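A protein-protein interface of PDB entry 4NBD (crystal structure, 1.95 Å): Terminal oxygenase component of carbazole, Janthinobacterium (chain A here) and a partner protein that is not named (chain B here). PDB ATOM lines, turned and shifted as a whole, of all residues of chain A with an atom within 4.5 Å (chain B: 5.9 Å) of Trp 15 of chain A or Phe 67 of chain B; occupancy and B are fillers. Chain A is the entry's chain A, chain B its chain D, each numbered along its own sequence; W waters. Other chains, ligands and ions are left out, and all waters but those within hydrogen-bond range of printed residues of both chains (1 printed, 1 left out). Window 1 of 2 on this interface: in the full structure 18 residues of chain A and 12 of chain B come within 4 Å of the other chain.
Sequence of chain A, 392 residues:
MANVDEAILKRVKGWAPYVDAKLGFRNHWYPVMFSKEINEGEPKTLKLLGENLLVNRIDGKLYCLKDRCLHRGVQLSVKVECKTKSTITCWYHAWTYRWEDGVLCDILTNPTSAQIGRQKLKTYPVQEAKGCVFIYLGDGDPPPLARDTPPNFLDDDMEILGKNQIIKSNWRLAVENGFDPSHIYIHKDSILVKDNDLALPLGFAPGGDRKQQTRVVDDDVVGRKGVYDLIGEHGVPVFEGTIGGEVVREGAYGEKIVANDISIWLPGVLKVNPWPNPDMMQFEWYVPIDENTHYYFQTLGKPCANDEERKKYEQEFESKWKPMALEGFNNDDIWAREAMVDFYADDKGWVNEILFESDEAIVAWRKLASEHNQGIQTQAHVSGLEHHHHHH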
ATOM      1  N   ARG A  11     -11.802 -13.589  13.897  1.00  0.00           N
ATOM      2  CA  ARG A  11     -12.365 -13.225  12.597  1.00  0.00           C
ATOM      3  C   ARG A  11     -11.368 -12.585  11.624  1.00  0.00           C
ATOM      4  O   ARG A  11     -11.400 -12.858  10.426  1.00  0.00           O
ATOM      5  CB  ARG A  11     -13.534 -12.258  12.787  1.00  0.00           C
ATOM      6  CG  ARG A  11     -14.860 -12.905  13.126  1.00  0.00           C
ATOM      7  CD  ARG A  11     -15.893 -11.832  13.425  1.00  0.00           C
ATOM      8  NE  ARG A  11     -17.252 -12.360  13.419  1.00  0.00           N
ATOM      9  CZ  ARG A  11     -17.939 -12.644  12.318  1.00  0.00           C
ATOM     10  NH1 ARG A  11     -17.396 -12.451  11.120  1.00  0.00           N
ATOM     11  NH2 ARG A  11     -19.171 -13.132  12.418  1.00  0.00           N
ATOM     12  N   VAL A  12     -10.492 -11.727  12.136  1.00  0.00           N
ATOM     13  CA  VAL A  12      -9.521 -11.037  11.285  1.00  0.00           C
ATOM     14  C   VAL A  12      -8.203 -11.791  11.149  1.00  0.00           C
ATOM     15  O   VAL A  12      -7.140 -11.291  11.526  1.00  0.00           O
ATOM     16  CB  VAL A  12      -9.248  -9.615  11.815  1.00  0.00           C
ATOM     17  CG1 VAL A  12     -10.486  -8.755  11.632  1.00  0.00           C
ATOM     18  CG2 VAL A  12      -8.868  -9.668  13.287  1.00  0.00           C
ATOM     19  N   LYS A  13      -8.287 -12.991  10.586  1.00  0.00           N
ATOM     20  CA  LYS A  13      -7.128 -13.856  10.395  1.00  0.00           C
ATOM     21  C   LYS A  13      -6.015 -13.235   9.556  1.00  0.00           C
ATOM     22  O   LYS A  13      -4.856 -13.613   9.678  1.00  0.00           O
ATOM     23  CB  LYS A  13      -7.572 -15.175   9.755  1.00  0.00           C
ATOM     24  CG  LYS A  13      -8.529 -15.983  10.618  1.00  0.00           C
ATOM     25  CD  LYS A  13      -8.984 -17.251   9.901  1.00  0.00           C
ATOM     26  CE  LYS A  13      -9.839 -18.123  10.815  1.00  0.00           C
ATOM     27  NZ  LYS A  13     -11.015 -17.382  11.370  1.00  0.00           N
ATOM     28  N   GLY A  14      -6.368 -12.282   8.704  1.00  0.00           N
ATOM     29  CA  GLY A  14      -5.363 -11.652   7.872  1.00  0.00           C
ATOM     30  C   GLY A  14      -4.455 -10.693   8.620  1.00  0.00           C
ATOM     31  O   GLY A  14      -3.313 -10.472   8.209  1.00  0.00           O
ATOM     32  N   TRP A  15      -4.938 -10.139   9.730  1.00  0.00           N
ATOM     33  CA  TRP A  15      -4.143  -9.176  10.484  1.00  0.00           C
ATOM     34  C   TRP A  15      -4.559  -8.999  11.948  1.00  0.00           C
ATOM     35  O   TRP A  15      -4.720  -7.873  12.429  1.00  0.00           O
ATOM     36  CB  TRP A  15      -4.189  -7.832   9.750  1.00  0.00           C
ATOM     37  CG  TRP A  15      -5.579  -7.418   9.303  1.00  0.00           C
ATOM     38  CD1 TRP A  15      -6.572  -6.897  10.081  1.00  0.00           C
ATOM     39  CD2 TRP A  15      -6.114  -7.495   7.974  1.00  0.00           C
ATOM     40  NE1 TRP A  15      -7.689  -6.641   9.322  1.00  0.00           N
ATOM     41  CE2 TRP A  15      -7.436  -7.000   8.025  1.00  0.00           C
ATOM     42  CE3 TRP A  15      -5.604  -7.934   6.742  1.00  0.00           C
ATOM     43  CZ2 TRP A  15      -8.258  -6.930   6.892  1.00  0.00           C
ATOM     44  CZ3 TRP A  15      -6.420  -7.864   5.619  1.00  0.00           C
ATOM     45  CH2 TRP A  15      -7.734  -7.366   5.703  1.00  0.00           C
ATOM     46  N   ALA A  16      -4.707 -10.112  12.659  1.00  0.00           N
ATOM     47  CA  ALA A  16      -5.109 -10.080  14.065  1.00  0.00           C
ATOM     48  C   ALA A  16      -4.165  -9.287  14.978  1.00  0.00           C
ATOM     49  O   ALA A  16      -4.616  -8.560  15.858  1.00  0.00           O
ATOM     50  CB  ALA A  16      -5.275 -11.514  14.594  1.00  0.00           C
ATOM     51  N   PRO A  17      -2.841  -9.423  14.792  1.00  0.00           N
ATOM     52  CA  PRO A  17      -1.912  -8.674  15.650  1.00  0.00           C
ATOM     53  C   PRO A  17      -2.111  -7.160  15.536  1.00  0.00           C
ATOM     54  O   PRO A  17      -2.022  -6.438  16.528  1.00  0.00           O
ATOM     55  CB  PRO A  17      -0.541  -9.112  15.138  1.00  0.00           C
ATOM     56  CG  PRO A  17      -0.806 -10.518  14.645  1.00  0.00           C
ATOM     57  CD  PRO A  17      -2.107 -10.345  13.909  1.00  0.00           C
ATOM     58  N   TYR A  18      -2.380  -6.692  14.323  1.00  0.00           N
ATOM     59  CA  TYR A  18      -2.587  -5.266  14.071  1.00  0.00           C
ATOM     60  C   TYR A  18      -3.858  -4.766  14.765  1.00  0.00           C
ATOM     61  O   TYR A  18      -3.865  -3.699  15.380  1.00  0.00           O
ATOM     62  CB  TYR A  18      -2.691  -5.025  12.564  1.00  0.00           C
ATOM     63  CG  TYR A  18      -2.995  -3.595  12.170  1.00  0.00           C
ATOM     64  CD1 TYR A  18      -2.023  -2.602  12.254  1.00  0.00           C
ATOM     65  CD2 TYR A  18      -4.246  -3.247  11.670  1.00  0.00           C
ATOM     66  CE1 TYR A  18      -2.284  -1.295  11.836  1.00  0.00           C
ATOM     67  CE2 TYR A  18      -4.521  -1.941  11.249  1.00  0.00           C
ATOM     68  CZ  TYR A  18      -3.534  -0.976  11.330  1.00  0.00           C
ATOM     69  OH  TYR A  18      -3.783   0.294  10.862  1.00  0.00           O
ATOM     70  N   VAL A  19      -4.935  -5.543  14.655  1.00  0.00           N
ATOM     71  CA  VAL A  19      -6.202  -5.183  15.277  1.00  0.00           C
ATOM     72  C   VAL A  19      -6.062  -5.213  16.797  1.00  0.00           C
ATOM     73  O   VAL A  19      -6.707  -4.442  17.510  1.00  0.00           O
ATOM     74  CB  VAL A  19      -7.327  -6.152  14.836  1.00  0.00           C
ATOM     75  CG1 VAL A  19      -8.599  -5.886  15.624  1.00  0.00           C
ATOM     76  CG2 VAL A  19      -7.591  -5.979  13.356  1.00  0.00           C
ATOM     77  N   GLU A 353     -16.403  -3.049   8.261  1.00  0.00           N
ATOM     78  CA  GLU A 353     -15.967  -2.143   7.190  1.00  0.00           C
ATOM     79  C   GLU A 353     -16.181  -2.818   5.835  1.00  0.00           C
ATOM     80  O   GLU A 353     -16.043  -4.030   5.726  1.00  0.00           O
ATOM     81  CB  GLU A 353     -14.470  -1.829   7.345  1.00  0.00           C
ATOM     82  CG  GLU A 353     -13.596  -3.087   7.244  1.00  0.00           C
ATOM     83  CD  GLU A 353     -12.126  -2.862   7.597  1.00  0.00           C
ATOM     84  OE1 GLU A 353     -11.767  -1.761   8.077  1.00  0.00           O
ATOM     85  OE2 GLU A 353     -11.329  -3.807   7.400  1.00  0.00           O
ATOM     86  N   VAL A 363      -4.622  -2.822   3.184  1.00  0.00           N
ATOM     87  CA  VAL A 363      -4.548  -4.245   3.496  1.00  0.00           C
ATOM     88  C   VAL A 363      -3.086  -4.697   3.549  1.00  0.00           C
ATOM     89  O   VAL A 363      -2.693  -5.456   4.433  1.00  0.00           O
ATOM     90  CB  VAL A 363      -5.321  -5.075   2.440  1.00  0.00           C
ATOM     91  CG1 VAL A 363      -4.920  -6.555   2.518  1.00  0.00           C
ATOM     92  CG2 VAL A 363      -6.817  -4.925   2.684  1.00  0.00           C
ATOM     93  N   ARG A 366      -1.631  -3.471   6.796  1.00  0.00           N
ATOM     94  CA  ARG A 366      -2.098  -4.224   7.949  1.00  0.00           C
ATOM     95  C   ARG A 366      -1.355  -5.552   8.055  1.00  0.00           C
ATOM     96  O   ARG A 366      -1.007  -5.983   9.154  1.00  0.00           O
ATOM     97  CB  ARG A 366      -3.608  -4.483   7.865  1.00  0.00           C
ATOM     98  CG  ARG A 366      -4.470  -3.216   7.984  1.00  0.00           C
ATOM     99  CD  ARG A 366      -5.954  -3.570   7.984  1.00  0.00           C
ATOM    100  NE  ARG A 366      -6.813  -2.387   8.039  1.00  0.00           N
ATOM    101  CZ  ARG A 366      -8.127  -2.412   7.837  1.00  0.00           C
ATOM    102  NH1 ARG A 366      -8.729  -3.563   7.563  1.00  0.00           N
ATOM    103  NH2 ARG A 366      -8.838  -1.292   7.921  1.00  0.00           N
ATOM    104  N   LYS A 367      -1.124  -6.200   6.916  1.00  0.00           N
ATOM    105  CA  LYS A 367      -0.415  -7.477   6.912  1.00  0.00           C
ATOM    106  C   LYS A 367       1.068  -7.288   7.254  1.00  0.00           C
ATOM    107  O   LYS A 367       1.619  -8.039   8.048  1.00  0.00           O
ATOM    108  CB  LYS A 367      -0.596  -8.168   5.561  1.00  0.00           C
ATOM    109  CG  LYS A 367      -2.026  -8.654   5.367  1.00  0.00           C
ATOM    110  CD  LYS A 367      -2.213  -9.457   4.088  1.00  0.00           C
ATOM    111  CE  LYS A 367      -3.623 -10.035   4.031  1.00  0.00           C
ATOM    112  NZ  LYS A 367      -3.892 -10.715   2.730  1.00  0.00           N
ATOM    113  N   SER A 370       1.294  -6.565  10.979  1.00  0.00           N
ATOM    114  CA  SER A 370       1.011  -7.770  11.763  1.00  0.00           C
ATOM    115  C   SER A 370       2.178  -8.756  11.746  1.00  0.00           C
ATOM    116  O   SER A 370       2.456  -9.417  12.739  1.00  0.00           O
ATOM    117  CB  SER A 370      -0.227  -8.510  11.225  1.00  0.00           C
ATOM    118  OG  SER A 370      -1.413  -7.742  11.351  1.00  0.00           O
ATOM    119  N   GLY B  49     -15.904  -7.262   0.467  1.00  0.00           N
ATOM    120  CA  GLY B  49     -14.699  -6.454   0.389  1.00  0.00           C
ATOM    121  C   GLY B  49     -13.832  -6.732  -0.817  1.00  0.00           C
ATOM    122  O   GLY B  49     -14.322  -6.793  -1.949  1.00  0.00           O
ATOM    123  N   ILE B  50     -12.535  -6.906  -0.575  1.00  0.00           N
ATOM    124  CA  ILE B  50     -11.592  -7.160  -1.659  1.00  0.00           C
ATOM    125  C   ILE B  50     -10.711  -8.375  -1.395  1.00  0.00           C
ATOM    126  O   ILE B  50      -9.672  -8.553  -2.035  1.00  0.00           O
ATOM    127  CB  ILE B  50     -10.680  -5.935  -1.890  1.00  0.00           C
ATOM    128  CG1 ILE B  50      -9.867  -5.637  -0.625  1.00  0.00           C
ATOM    129  CG2 ILE B  50     -11.526  -4.736  -2.301  1.00  0.00           C
ATOM    130  CD1 ILE B  50      -8.897  -4.448  -0.770  1.00  0.00           C
ATOM    131  N   ALA B  51     -11.137  -9.217  -0.462  1.00  0.00           N
ATOM    132  CA  ALA B  51     -10.379 -10.411  -0.114  1.00  0.00           C
ATOM    133  C   ALA B  51     -10.540 -11.530  -1.141  1.00  0.00           C
ATOM    134  O   ALA B  51     -11.506 -11.559  -1.911  1.00  0.00           O
ATOM    135  CB  ALA B  51     -10.809 -10.908   1.250  1.00  0.00           C
ATOM    136  N   SER B  52      -9.578 -12.448  -1.138  1.00  0.00           N
ATOM    137  CA  SER B  52      -9.583 -13.601  -2.032  1.00  0.00           C
ATOM    138  C   SER B  52     -10.050 -14.806  -1.231  1.00  0.00           C
ATOM    139  O   SER B  52      -9.357 -15.257  -0.317  1.00  0.00           O
ATOM    140  CB  SER B  52      -8.173 -13.868  -2.569  1.00  0.00           C
ATOM    141  OG  SER B  52      -8.115 -15.116  -3.236  1.00  0.00           O
ATOM    142  N   CYS B  65     -14.138 -16.286   4.641  1.00  0.00           N
ATOM    143  CA  CYS B  65     -13.259 -15.218   4.171  1.00  0.00           C
ATOM    144  C   CYS B  65     -12.173 -14.934   5.210  1.00  0.00           C
ATOM    145  O   CYS B  65     -12.455 -14.802   6.398  1.00  0.00           O
ATOM    146  CB  CYS B  65     -14.073 -13.949   3.907  1.00  0.00           C
ATOM    147  SG  CYS B  65     -13.090 -12.564   3.293  1.00  0.00           S
ATOM    148  N   PRO B  66     -10.910 -14.837   4.766  1.00  0.00           N
ATOM    149  CA  PRO B  66      -9.769 -14.571   5.651  1.00  0.00           C
ATOM    150  C   PRO B  66      -9.699 -13.162   6.234  1.00  0.00           C
ATOM    151  O   PRO B  66      -8.986 -12.927   7.211  1.00  0.00           O
ATOM    152  CB  PRO B  66      -8.569 -14.879   4.757  1.00  0.00           C
ATOM    153  CG  PRO B  66      -9.054 -14.468   3.405  1.00  0.00           C
ATOM    154  CD  PRO B  66     -10.455 -15.051   3.379  1.00  0.00           C
ATOM    155  N   PHE B  67     -10.440 -12.230   5.644  1.00  0.00           N
ATOM    156  CA  PHE B  67     -10.431 -10.842   6.109  1.00  0.00           C
ATOM    157  C   PHE B  67     -11.227 -10.563   7.379  1.00  0.00           C
ATOM    158  O   PHE B  67     -10.655 -10.169   8.397  1.00  0.00           O
ATOM    159  CB  PHE B  67     -10.940  -9.912   5.003  1.00  0.00           C
ATOM    160  CG  PHE B  67      -9.878  -9.461   4.038  1.00  0.00           C
ATOM    161  CD1 PHE B  67      -8.728 -10.218   3.829  1.00  0.00           C
ATOM    162  CD2 PHE B  67     -10.051  -8.286   3.307  1.00  0.00           C
ATOM    163  CE1 PHE B  67      -7.765  -9.813   2.901  1.00  0.00           C
ATOM    164  CE2 PHE B  67      -9.096  -7.873   2.378  1.00  0.00           C
ATOM    165  CZ  PHE B  67      -7.951  -8.638   2.174  1.00  0.00           C
ATOM    166  N   HIS B  68     -12.542 -10.765   7.317  1.00  0.00           N
ATOM    167  CA  HIS B  68     -13.404 -10.477   8.459  1.00  0.00           C
ATOM    168  C   HIS B  68     -14.195 -11.661   9.020  1.00  0.00           C
ATOM    169  O   HIS B  68     -14.993 -11.492   9.944  1.00  0.00           O
ATOM    170  CB  HIS B  68     -14.374  -9.351   8.086  1.00  0.00           C
ATOM    171  CG  HIS B  68     -13.711  -8.159   7.465  1.00  0.00           C
ATOM    172  ND1 HIS B  68     -13.918  -7.795   6.151  1.00  0.00           N
ATOM    173  CD2 HIS B  68     -12.854  -7.244   7.977  1.00  0.00           C
ATOM    174  CE1 HIS B  68     -13.217  -6.707   5.881  1.00  0.00           C
ATOM    175  NE2 HIS B  68     -12.562  -6.351   6.973  1.00  0.00           N
ATOM    176  N   GLY B  69     -13.988 -12.852   8.470  1.00  0.00           N
ATOM    177  CA  GLY B  69     -14.698 -14.011   8.979  1.00  0.00           C
ATOM    178  C   GLY B  69     -16.043 -14.297   8.332  1.00  0.00           C
ATOM    179  O   GLY B  69     -16.741 -15.231   8.735  1.00  0.00           O
HETATM  180  O   HOH W   1     -11.611 -15.147   9.140  1.00  0.00           O
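Water W1 lies within hydrogen-bond range of O of Arg 11 of chain A, O of Cys 65 of chain B, NZ of Lys 13 of chain A and N of Gly 69 of chain B.
O of His 68 of chain B sits at hydrogen-bond distance from NH1 of Arg 11 of chain A, at 2.8 Å. O of Arg 11 of chain A lies within hydrogen-bond range of N of Gly 69 of chain B (3.2 Å). O of Pro 66 of chain B lies within hydrogen-bond range of N of Lys 13 of chain A, at 3.4 Å. The backbone NH of Gly 14 of chain A sits at hydrogen-bond distance from the backbone carbonyl oxygen of Pro 66 of chain B, 3.1 Å away. NE2 of His 68 of chain B sits at hydrogen-bond distance from OE2 of Glu 353 of chain A (2.9 Å). The backbone carbonyl oxygen (O) of Phe 67 of chain B sits close to the backbone carbonyl oxygen (O) of Arg 11 of chain A (3.5 Å).
Phe 67 of chain B touches Val 12 of chain A (O to CA, 3.2 Å). CH2 of Trp 15 of chain A touches CG of Phe 67 of chain B, 3.4 Å away. CZ of Phe 67 of chain B touches CG1 of Val 363 of chain A (3.7 Å). Phe 67 of chain B touches Lys 367 of chain A (CE1 to NZ, 3.98 Å).
O of Trp 15 of chain A lies close to OG of Ser 370 of chain A. The side-chain carboxylate (OE2) of Glu 353 of chain A lies within salt-bridge range of the guanidinium group (NH1) of Arg 366 of chain A (2.6 Å). SG of Cys 65 of chain B lies close to N of Phe 67 of chain B, at 3.6 Å.
Of the printed residues of chain B, Arg 11 of chain A touches Phe 67 (3.5 Å), His 68 (2.8 Å) and Gly 69 (3.2 Å). Of chain B, only Phe 67 (3.4 Å) comes within 4 Å of Trp 15 of chain A. Pro 17 of chain A touches none of the printed residues of chain B. Of the printed residues of chain A, Pro 66 of chain B touches Lys 13 (3.4 Å) and Gly 14 (3.1 Å).
Of the 9 printed residues of chain B, 4 touch a printed residue of chain A. Hydrophobic or aromatic side chains of chain B that line the printed part of chain A: Phe 67 and His 68. Among the printed residues, no Asp or Glu carboxylate lies within 4 Å of a Lys or Arg side-chain nitrogen of the other chain.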
